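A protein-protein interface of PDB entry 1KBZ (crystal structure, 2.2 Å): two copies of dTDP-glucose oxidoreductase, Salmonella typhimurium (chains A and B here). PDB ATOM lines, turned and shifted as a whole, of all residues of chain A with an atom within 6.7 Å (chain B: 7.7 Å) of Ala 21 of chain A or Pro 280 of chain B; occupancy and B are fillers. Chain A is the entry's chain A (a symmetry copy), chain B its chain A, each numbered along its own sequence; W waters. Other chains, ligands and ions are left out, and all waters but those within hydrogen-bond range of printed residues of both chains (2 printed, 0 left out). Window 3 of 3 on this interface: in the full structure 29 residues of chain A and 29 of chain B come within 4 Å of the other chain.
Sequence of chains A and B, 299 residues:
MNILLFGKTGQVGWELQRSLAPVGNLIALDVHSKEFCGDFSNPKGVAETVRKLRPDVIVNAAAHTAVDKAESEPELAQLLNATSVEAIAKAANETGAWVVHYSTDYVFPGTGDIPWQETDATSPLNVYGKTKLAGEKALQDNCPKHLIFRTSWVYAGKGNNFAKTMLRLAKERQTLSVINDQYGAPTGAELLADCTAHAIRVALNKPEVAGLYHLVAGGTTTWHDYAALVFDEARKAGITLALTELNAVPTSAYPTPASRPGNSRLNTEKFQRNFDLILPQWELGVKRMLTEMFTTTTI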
ATOM      1  N   ILE A   3      -4.181  23.048  -1.132  1.00  0.00           N
ATOM      2  CA  ILE A   3      -5.203  23.526  -0.218  1.00  0.00           C
ATOM      3  C   ILE A   3      -4.629  24.585   0.668  1.00  0.00           C
ATOM      4  O   ILE A   3      -3.535  24.437   1.174  1.00  0.00           O
ATOM      5  CB  ILE A   3      -5.710  22.376   0.715  1.00  0.00           C
ATOM      6  CG1 ILE A   3      -6.393  21.319  -0.133  1.00  0.00           C
ATOM      7  CG2 ILE A   3      -6.623  22.941   1.810  1.00  0.00           C
ATOM      8  CD1 ILE A   3      -6.733  19.972   0.600  1.00  0.00           C
ATOM      9  N   LEU A  16      -8.172  20.485  11.334  1.00  0.00           N
ATOM     10  CA  LEU A  16      -8.061  20.553   9.866  1.00  0.00           C
ATOM     11  C   LEU A  16      -6.645  20.373   9.374  1.00  0.00           C
ATOM     12  O   LEU A  16      -6.446  19.819   8.317  1.00  0.00           O
ATOM     13  CB  LEU A  16      -8.632  21.856   9.303  1.00  0.00           C
ATOM     14  CG  LEU A  16     -10.133  21.985   9.345  1.00  0.00           C
ATOM     15  CD1 LEU A  16     -10.598  23.448   9.371  1.00  0.00           C
ATOM     16  CD2 LEU A  16     -10.766  21.163   8.188  1.00  0.00           C
ATOM     17  N   GLN A  17      -5.653  20.814  10.140  1.00  0.00           N
ATOM     18  CA  GLN A  17      -4.280  20.565   9.780  1.00  0.00           C
ATOM     19  C   GLN A  17      -4.088  19.065   9.616  1.00  0.00           C
ATOM     20  O   GLN A  17      -3.319  18.603   8.781  1.00  0.00           O
ATOM     21  CB  GLN A  17      -3.294  21.102  10.819  1.00  0.00           C
ATOM     22  CG  GLN A  17      -3.213  22.684  10.900  1.00  0.00           C
ATOM     23  CD  GLN A  17      -2.076  23.140  11.777  1.00  0.00           C
ATOM     24  OE1 GLN A  17      -2.266  23.873  12.737  1.00  0.00           O
ATOM     25  NE2 GLN A  17      -0.907  22.664  11.481  1.00  0.00           N
ATOM     26  N   ARG A  18      -4.766  18.299  10.434  1.00  0.00           N
ATOM     27  CA  ARG A  18      -4.684  16.854  10.369  1.00  0.00           C
ATOM     28  C   ARG A  18      -5.553  16.326   9.220  1.00  0.00           C
ATOM     29  O   ARG A  18      -5.035  15.632   8.366  1.00  0.00           O
ATOM     30  CB  ARG A  18      -5.122  16.213  11.716  1.00  0.00           C
ATOM     31  CG  ARG A  18      -5.307  14.718  11.683  1.00  0.00           C
ATOM     32  CD  ARG A  18      -6.049  14.087  12.891  1.00  0.00           C
ATOM     33  NE  ARG A  18      -7.326  14.727  13.153  1.00  0.00           N
ATOM     34  CZ  ARG A  18      -8.394  14.665  12.364  1.00  0.00           C
ATOM     35  NH1 ARG A  18      -8.390  13.939  11.249  1.00  0.00           N
ATOM     36  NH2 ARG A  18      -9.500  15.299  12.733  1.00  0.00           N
ATOM     37  N   SER A  19      -6.835  16.649   9.215  1.00  0.00           N
ATOM     38  CA  SER A  19      -7.792  16.034   8.284  1.00  0.00           C
ATOM     39  C   SER A  19      -7.525  16.369   6.818  1.00  0.00           C
ATOM     40  O   SER A  19      -7.785  15.553   5.951  1.00  0.00           O
ATOM     41  CB  SER A  19      -9.255  16.449   8.599  1.00  0.00           C
ATOM     42  OG  SER A  19      -9.433  17.825   8.290  1.00  0.00           O
ATOM     43  N   LEU A  20      -6.999  17.564   6.564  1.00  0.00           N
ATOM     44  CA  LEU A  20      -6.762  18.011   5.208  1.00  0.00           C
ATOM     45  C   LEU A  20      -5.430  17.481   4.677  1.00  0.00           C
ATOM     46  O   LEU A  20      -5.194  17.541   3.483  1.00  0.00           O
ATOM     47  CB  LEU A  20      -6.758  19.560   5.143  1.00  0.00           C
ATOM     48  CG  LEU A  20      -8.062  20.273   5.499  1.00  0.00           C
ATOM     49  CD1 LEU A  20      -7.897  21.732   5.356  1.00  0.00           C
ATOM     50  CD2 LEU A  20      -9.225  19.785   4.599  1.00  0.00           C
ATOM     51  N   ALA A  21      -4.559  16.966   5.553  1.00  0.00           N
ATOM     52  CA  ALA A  21      -3.208  16.572   5.114  1.00  0.00           C
ATOM     53  C   ALA A  21      -3.105  15.534   3.966  1.00  0.00           C
ATOM     54  O   ALA A  21      -2.230  15.662   3.147  1.00  0.00           O
ATOM     55  CB  ALA A  21      -2.345  16.159   6.295  1.00  0.00           C
ATOM     56  N   PRO A  22      -3.918  14.476   3.942  1.00  0.00           N
ATOM     57  CA  PRO A  22      -3.877  13.580   2.810  1.00  0.00           C
ATOM     58  C   PRO A  22      -4.779  14.013   1.650  1.00  0.00           C
ATOM     59  O   PRO A  22      -4.626  13.422   0.618  1.00  0.00           O
ATOM     60  CB  PRO A  22      -4.326  12.255   3.406  1.00  0.00           C
ATOM     61  CG  PRO A  22      -5.283  12.643   4.424  1.00  0.00           C
ATOM     62  CD  PRO A  22      -4.779  13.944   5.010  1.00  0.00           C
ATOM     63  N   VAL A  23      -5.604  15.054   1.810  1.00  0.00           N
ATOM     64  CA  VAL A  23      -6.515  15.484   0.771  1.00  0.00           C
ATOM     65  C   VAL A  23      -5.795  16.224  -0.336  1.00  0.00           C
ATOM     66  O   VAL A  23      -6.126  16.046  -1.485  1.00  0.00           O
ATOM     67  CB  VAL A  23      -7.698  16.313   1.296  1.00  0.00           C
ATOM     68  CG1 VAL A  23      -8.638  16.645   0.183  1.00  0.00           C
ATOM     69  CG2 VAL A  23      -8.456  15.458   2.333  1.00  0.00           C
ATOM     70  N   GLY A  24      -4.792  17.002   0.034  1.00  0.00           N
ATOM     71  CA  GLY A  24      -3.935  17.634  -0.934  1.00  0.00           C
ATOM     72  C   GLY A  24      -2.808  18.318  -0.192  1.00  0.00           C
ATOM     73  O   GLY A  24      -2.765  18.291   1.033  1.00  0.00           O
ATOM     74  N   ASN A  25      -1.924  18.940  -0.953  1.00  0.00           N
ATOM     75  CA  ASN A  25      -0.807  19.708  -0.417  1.00  0.00           C
ATOM     76  C   ASN A  25      -1.287  20.896   0.393  1.00  0.00           C
ATOM     77  O   ASN A  25      -1.857  21.826  -0.143  1.00  0.00           O
ATOM     78  CB  ASN A  25       0.078  20.143  -1.571  1.00  0.00           C
ATOM     79  CG  ASN A  25       0.787  18.975  -2.186  1.00  0.00           C
ATOM     80  OD1 ASN A  25       1.595  18.318  -1.521  1.00  0.00           O
ATOM     81  ND2 ASN A  25       0.460  18.662  -3.427  1.00  0.00           N
ATOM     82  N   LEU A  26      -1.080  20.808   1.706  1.00  0.00           N
ATOM     83  CA  LEU A  26      -1.603  21.784   2.652  1.00  0.00           C
ATOM     84  C   LEU A  26      -0.633  22.923   3.021  1.00  0.00           C
ATOM     85  O   LEU A  26       0.488  22.683   3.444  1.00  0.00           O
ATOM     86  CB  LEU A  26      -2.000  21.078   3.940  1.00  0.00           C
ATOM     87  CG  LEU A  26      -2.654  21.949   4.995  1.00  0.00           C
ATOM     88  CD1 LEU A  26      -3.963  22.514   4.536  1.00  0.00           C
ATOM     89  CD2 LEU A  26      -2.884  21.084   6.223  1.00  0.00           C
ATOM     90  N   ALA B 185      10.007   5.296   7.693  1.00  0.00           N
ATOM     91  CA  ALA B 185       9.246   6.514   7.877  1.00  0.00           C
ATOM     92  C   ALA B 185       8.215   6.312   9.002  1.00  0.00           C
ATOM     93  O   ALA B 185       7.313   5.482   8.880  1.00  0.00           O
ATOM     94  CB  ALA B 185       8.580   6.863   6.604  1.00  0.00           C
ATOM     95  N   PRO B 186       8.391   6.976  10.134  1.00  0.00           N
ATOM     96  CA  PRO B 186       7.405   6.893  11.214  1.00  0.00           C
ATOM     97  C   PRO B 186       6.056   7.306  10.688  1.00  0.00           C
ATOM     98  O   PRO B 186       5.948   8.323  10.045  1.00  0.00           O
ATOM     99  CB  PRO B 186       7.911   7.915  12.228  1.00  0.00           C
ATOM    100  CG  PRO B 186       9.380   7.971  11.979  1.00  0.00           C
ATOM    101  CD  PRO B 186       9.549   7.799  10.519  1.00  0.00           C
ATOM    102  N   THR B 187       5.030   6.518  10.952  1.00  0.00           N
ATOM    103  CA  THR B 187       3.726   6.809  10.377  1.00  0.00           C
ATOM    104  C   THR B 187       2.703   6.928  11.482  1.00  0.00           C
ATOM    105  O   THR B 187       2.563   6.035  12.321  1.00  0.00           O
ATOM    106  CB  THR B 187       3.383   5.698   9.401  1.00  0.00           C
ATOM    107  OG1 THR B 187       4.360   5.699   8.332  1.00  0.00           O
ATOM    108  CG2 THR B 187       2.077   5.951   8.764  1.00  0.00           C
ATOM    109  N   LEU B 191      -2.623   9.631  10.381  1.00  0.00           N
ATOM    110  CA  LEU B 191      -2.554   9.480   8.926  1.00  0.00           C
ATOM    111  C   LEU B 191      -3.183   8.170   8.465  1.00  0.00           C
ATOM    112  O   LEU B 191      -3.987   8.131   7.502  1.00  0.00           O
ATOM    113  CB  LEU B 191      -1.109   9.618   8.434  1.00  0.00           C
ATOM    114  CG  LEU B 191      -1.020   9.433   6.924  1.00  0.00           C
ATOM    115  CD1 LEU B 191      -1.607  10.633   6.212  1.00  0.00           C
ATOM    116  CD2 LEU B 191       0.411   9.182   6.490  1.00  0.00           C
ATOM    117  N   ASP B 194      -7.072   8.403   8.789  1.00  0.00           N
ATOM    118  CA  ASP B 194      -7.732   9.281   7.841  1.00  0.00           C
ATOM    119  C   ASP B 194      -7.668   8.708   6.403  1.00  0.00           C
ATOM    120  O   ASP B 194      -8.649   8.733   5.672  1.00  0.00           O
ATOM    121  CB  ASP B 194      -7.147  10.692   7.966  1.00  0.00           C
ATOM    122  CG  ASP B 194      -7.511  11.358   9.292  1.00  0.00           C
ATOM    123  OD1 ASP B 194      -6.772  12.275   9.811  1.00  0.00           O
ATOM    124  OD2 ASP B 194      -8.509  10.970   9.908  1.00  0.00           O
ATOM    125  N   CYS B 195      -6.514   8.187   6.001  1.00  0.00           N
ATOM    126  CA  CYS B 195      -6.353   7.591   4.685  1.00  0.00           C
ATOM    127  C   CYS B 195      -7.319   6.434   4.543  1.00  0.00           C
ATOM    128  O   CYS B 195      -7.928   6.225   3.477  1.00  0.00           O
ATOM    129  CB  CYS B 195      -4.930   7.087   4.513  1.00  0.00           C
ATOM    130  SG  CYS B 195      -3.824   8.435   4.100  1.00  0.00           S
ATOM    131  N   HIS B 198     -10.874   7.772   3.714  1.00  0.00           N
ATOM    132  CA  HIS B 198     -10.980   8.151   2.299  1.00  0.00           C
ATOM    133  C   HIS B 198     -10.953   6.892   1.362  1.00  0.00           C
ATOM    134  O   HIS B 198     -11.719   6.785   0.439  1.00  0.00           O
ATOM    135  CB  HIS B 198      -9.885   9.150   1.921  1.00  0.00           C
ATOM    136  CG  HIS B 198     -10.032  10.448   2.648  1.00  0.00           C
ATOM    137  ND1 HIS B 198     -11.139  11.253   2.496  1.00  0.00           N
ATOM    138  CD2 HIS B 198      -9.262  11.036   3.589  1.00  0.00           C
ATOM    139  CE1 HIS B 198     -11.057  12.270   3.330  1.00  0.00           C
ATOM    140  NE2 HIS B 198      -9.927  12.164   4.004  1.00  0.00           N
ATOM    141  N   VAL B 216       2.656   4.661   4.185  1.00  0.00           N
ATOM    142  CA  VAL B 216       3.502   5.258   5.197  1.00  0.00           C
ATOM    143  C   VAL B 216       3.658   6.753   4.908  1.00  0.00           C
ATOM    144  O   VAL B 216       3.440   7.208   3.769  1.00  0.00           O
ATOM    145  CB  VAL B 216       4.938   4.601   5.209  1.00  0.00           C
ATOM    146  CG1 VAL B 216       4.902   3.150   5.683  1.00  0.00           C
ATOM    147  CG2 VAL B 216       5.595   4.692   3.819  1.00  0.00           C
ATOM    148  N   ALA B 217       3.987   7.529   5.944  1.00  0.00           N
ATOM    149  CA  ALA B 217       4.317   8.921   5.727  1.00  0.00           C
ATOM    150  C   ALA B 217       5.537   8.993   4.762  1.00  0.00           C
ATOM    151  O   ALA B 217       6.310   8.057   4.663  1.00  0.00           O
ATOM    152  CB  ALA B 217       4.637   9.612   7.040  1.00  0.00           C
ATOM    153  N   GLY B 218       5.646  10.084   4.019  1.00  0.00           N
ATOM    154  CA  GLY B 218       6.741  10.313   3.127  1.00  0.00           C
ATOM    155  C   GLY B 218       8.084  10.556   3.816  1.00  0.00           C
ATOM    156  O   GLY B 218       8.174  10.810   5.021  1.00  0.00           O
ATOM    157  N   GLY B 219       9.130  10.466   3.016  1.00  0.00           N
ATOM    158  CA  GLY B 219      10.499  10.629   3.491  1.00  0.00           C
ATOM    159  C   GLY B 219      11.101   9.359   4.051  1.00  0.00           C
ATOM    160  O   GLY B 219      10.629   8.258   3.867  1.00  0.00           O
ATOM    161  N   GLN B 272      -1.064   6.372  -3.562  1.00  0.00           N
ATOM    162  CA  GLN B 272      -1.241   7.764  -3.994  1.00  0.00           C
ATOM    163  C   GLN B 272      -2.057   7.957  -5.278  1.00  0.00           C
ATOM    164  O   GLN B 272      -2.952   8.803  -5.336  1.00  0.00           O
ATOM    165  CB  GLN B 272       0.138   8.434  -4.132  1.00  0.00           C
ATOM    166  CG  GLN B 272       0.844   8.635  -2.766  1.00  0.00           C
ATOM    167  CD  GLN B 272       2.268   9.154  -2.909  1.00  0.00           C
ATOM    168  OE1 GLN B 272       2.467  10.165  -3.541  1.00  0.00           O
ATOM    169  NE2 GLN B 272       3.252   8.448  -2.351  1.00  0.00           N
ATOM    170  N   LEU B 277      -4.651  10.538  -3.118  1.00  0.00           N
ATOM    171  CA  LEU B 277      -4.299  11.114  -1.840  1.00  0.00           C
ATOM    172  C   LEU B 277      -2.802  11.418  -1.704  1.00  0.00           C
ATOM    173  O   LEU B 277      -1.947  10.786  -2.346  1.00  0.00           O
ATOM    174  CB  LEU B 277      -4.698  10.169  -0.735  1.00  0.00           C
ATOM    175  CG  LEU B 277      -6.209   9.919  -0.546  1.00  0.00           C
ATOM    176  CD1 LEU B 277      -6.379   8.722   0.292  1.00  0.00           C
ATOM    177  CD2 LEU B 277      -6.873  11.126   0.103  1.00  0.00           C
ATOM    178  N   ILE B 278      -2.530  12.363  -0.806  1.00  0.00           N
ATOM    179  CA  ILE B 278      -1.190  12.840  -0.448  1.00  0.00           C
ATOM    180  C   ILE B 278      -0.729  12.145   0.822  1.00  0.00           C
ATOM    181  O   ILE B 278      -1.554  11.762   1.725  1.00  0.00           O
ATOM    182  CB  ILE B 278      -1.207  14.430  -0.294  1.00  0.00           C
ATOM    183  CG1 ILE B 278      -1.500  15.066  -1.641  1.00  0.00           C
ATOM    184  CG2 ILE B 278       0.101  15.020   0.232  1.00  0.00           C
ATOM    185  CD1 ILE B 278      -0.590  14.578  -2.747  1.00  0.00           C
ATOM    186  N   LEU B 279       0.569  11.846   0.859  1.00  0.00           N
ATOM    187  CA  LEU B 279       1.152  11.203   2.039  1.00  0.00           C
ATOM    188  C   LEU B 279       2.263  12.108   2.532  1.00  0.00           C
ATOM    189  O   LEU B 279       3.426  12.052   2.054  1.00  0.00           O
ATOM    190  CB  LEU B 279       1.610   9.807   1.734  1.00  0.00           C
ATOM    191  CG  LEU B 279       0.493   8.844   1.386  1.00  0.00           C
ATOM    192  CD1 LEU B 279       1.052   7.511   0.948  1.00  0.00           C
ATOM    193  CD2 LEU B 279      -0.428   8.618   2.524  1.00  0.00           C
ATOM    194  N   PRO B 280       1.930  13.000   3.447  1.00  0.00           N
ATOM    195  CA  PRO B 280       2.898  14.050   3.847  1.00  0.00           C
ATOM    196  C   PRO B 280       4.185  13.536   4.474  1.00  0.00           C
ATOM    197  O   PRO B 280       4.217  12.452   5.005  1.00  0.00           O
ATOM    198  CB  PRO B 280       2.108  14.921   4.825  1.00  0.00           C
ATOM    199  CG  PRO B 280       0.676  14.566   4.556  1.00  0.00           C
ATOM    200  CD  PRO B 280       0.663  13.096   4.165  1.00  0.00           C
ATOM    201  N   GLN B 281       5.243  14.339   4.397  1.00  0.00           N
ATOM    202  CA  GLN B 281       6.524  13.988   5.009  1.00  0.00           C
ATOM    203  C   GLN B 281       6.366  13.579   6.493  1.00  0.00           C
ATOM    204  O   GLN B 281       5.593  14.182   7.227  1.00  0.00           O
ATOM    205  CB  GLN B 281       7.488  15.154   4.851  1.00  0.00           C
ATOM    206  CG  GLN B 281       7.775  15.420   3.407  1.00  0.00           C
ATOM    207  CD  GLN B 281       8.340  14.172   2.771  1.00  0.00           C
ATOM    208  OE1 GLN B 281       9.306  13.605   3.287  1.00  0.00           O
ATOM    209  NE2 GLN B 281       7.713  13.705   1.695  1.00  0.00           N
ATOM    210  N   TRP B 282       7.142  12.596   6.937  1.00  0.00           N
ATOM    211  CA  TRP B 282       6.974  12.042   8.263  1.00  0.00           C
ATOM    212  C   TRP B 282       7.073  13.011   9.427  1.00  0.00           C
ATOM    213  O   TRP B 282       6.465  12.795  10.462  1.00  0.00           O
ATOM    214  CB  TRP B 282       7.931  10.850   8.479  1.00  0.00           C
ATOM    215  CG  TRP B 282       9.390  11.201   8.593  1.00  0.00           C
ATOM    216  CD1 TRP B 282      10.337  11.162   7.606  1.00  0.00           C
ATOM    217  CD2 TRP B 282      10.077  11.602   9.778  1.00  0.00           C
ATOM    218  NE1 TRP B 282      11.570  11.534   8.097  1.00  0.00           N
ATOM    219  CE2 TRP B 282      11.444  11.792   9.434  1.00  0.00           C
ATOM    220  CE3 TRP B 282       9.689  11.807  11.097  1.00  0.00           C
ATOM    221  CZ2 TRP B 282      12.394  12.204  10.356  1.00  0.00           C
ATOM    222  CZ3 TRP B 282      10.639  12.196  12.008  1.00  0.00           C
ATOM    223  CH2 TRP B 282      11.979  12.391  11.637  1.00  0.00           C
ATOM    224  N   GLU B 283       7.869  14.047   9.285  1.00  0.00           N
ATOM    225  CA  GLU B 283       8.111  14.976  10.384  1.00  0.00           C
ATOM    226  C   GLU B 283       6.853  15.688  10.820  1.00  0.00           C
ATOM    227  O   GLU B 283       6.719  16.037  11.975  1.00  0.00           O
ATOM    228  CB  GLU B 283       9.086  16.070   9.965  1.00  0.00           C
ATOM    229  CG  GLU B 283      10.529  15.645   9.858  1.00  0.00           C
ATOM    230  CD  GLU B 283      10.915  15.225   8.458  1.00  0.00           C
ATOM    231  OE1 GLU B 283      10.036  14.712   7.693  1.00  0.00           O
ATOM    232  OE2 GLU B 283      12.109  15.424   8.150  1.00  0.00           O
ATOM    233  N   LEU B 284       5.990  15.991   9.874  1.00  0.00           N
ATOM    234  CA  LEU B 284       4.812  16.819  10.171  1.00  0.00           C
ATOM    235  C   LEU B 284       3.978  16.163  11.251  1.00  0.00           C
ATOM    236  O   LEU B 284       3.631  16.780  12.247  1.00  0.00           O
ATOM    237  CB  LEU B 284       3.956  17.062   8.918  1.00  0.00           C
ATOM    238  CG  LEU B 284       4.442  18.193   7.972  1.00  0.00           C
ATOM    239  CD1 LEU B 284       4.468  17.755   6.524  1.00  0.00           C
ATOM    240  CD2 LEU B 284       3.554  19.501   8.107  1.00  0.00           C
ATOM    241  N   GLY B 285       3.740  14.877  11.053  1.00  0.00           N
ATOM    242  CA  GLY B 285       2.967  14.084  11.968  1.00  0.00           C
ATOM    243  C   GLY B 285       3.600  13.988  13.330  1.00  0.00           C
ATOM    244  O   GLY B 285       2.918  14.053  14.338  1.00  0.00           O
HETATM  245  O   HOH W   1      -4.099  12.874   8.643  1.00  0.00           O
HETATM  246  O   HOH W   2      -8.900  13.226   6.237  1.00  0.00           O
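The side-chain carboxylate (OD1) of Asp 194 of chain B lies within salt-bridge range of the guanidinium group (NH1) of Arg 18 of chain A.
The backbone carbonyl oxygen (O) of Pro 22 of chain A sits at hydrogen-bond distance from the backbone NH (N) of Ile 278 of chain B, 2.7 Å away.
The backbone carbonyl oxygen (O) of Leu 191 of chain B sits close to the side-chain sulfur (SG) of Cys 195 of chain B.
N of Gly 218 of chain B lies within hydrogen-bond range of O of Pro 280 of chain B, 2.9 Å away.
The backbone NH (N) of Leu 277 of chain B is in hydrogen-bond range of the backbone carbonyl oxygen (O) of Gln 272 of chain B (3.3 Å).
The backbone NH of Ile 3 of chain A is in hydrogen-bond range of the backbone carbonyl oxygen of Asn 25 of chain A (2.8 Å).
CG2 of Ile 278 of chain B touches O of Ala 21 of chain A, at 3.8 Å.
O of Ala 21 of chain A touches CG of Pro 280 of chain B (3.4 Å).
Cys 195 of chain B touches Pro 22 of chain A.
Leu 277 of chain B touches Pro 22 of chain A (CD2 to O, 3.3 Å).
His 198 of chain B touches Val 23 of chain A.
Gly 24 of chain A touches Ile 278 of chain B (CA to CG1, 3.6 Å).
N of Asn 25 of chain A touches CG1 of Ile 278 of chain B, 3.96 Å away.
Leu 16 of chain A touches none of the printed residues of chain B.
Leu 20 of chain A touches none of the printed residues of chain B.
Ala 21 of chain A touches just these residues of chain B: Ile 278 and Pro 280.
Of the printed residues of chain B, Pro 22 of chain A touches Cys 195, Leu 277 and Ile 278.
Of the printed residues of chain A, Asp 194 of chain B touches Arg 18.
Of the printed residues of chain A, Leu 277 of chain B touches Pro 22.
Pro 280 of chain B touches just one residue of chain A: Ala 21.
The nearest residue of chain B that does not touch Ala 21 of chain A is Leu 279 of chain B (5.3 Å).
The nearest residue of chain A that does not touch Pro 280 of chain B is Pro 22 of chain A (4.6 Å).
The nearest printed residue of chain B that does not touch Asn 25 of chain A is Leu 279 of chain B (7.0 Å).
Of the 21 printed residues of chain B, 6 touch a printed residue of chain A.
Printed residues of chain B that touch a printed residue of chain A: Asp 194, Cys 195, His 198, Leu 277, Ile 278 and Pro 280.
Hydrophobic or aromatic side chains of chain B within 4 Å of the printed part of chain A: His 198, Leu 277, Ile 278 and Pro 280.
Among the printed residues, Asp or Glu carboxylates within 4 Å of a Lys or Arg side-chain nitrogen of the other chain: Arg 18 of chain A with Asp 194 of chain B (2.7 Å).
No position is printed for both chains.
Of the 9 pairs that touch across the chains among the printed residues, none has its exchanged pair printed and touching as well.
Water W2 lies within hydrogen-bond range of the backbone carbonyl oxygen of Ser 19 of chain A (2.6 Å) and a ring nitrogen (NE2) of His 198 of chain B (2.7 Å).
Water W1 bridges O of Arg 18 of chain A (2.9 Å) and OD1 of Asp 194 of chain B (3.0 Å).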
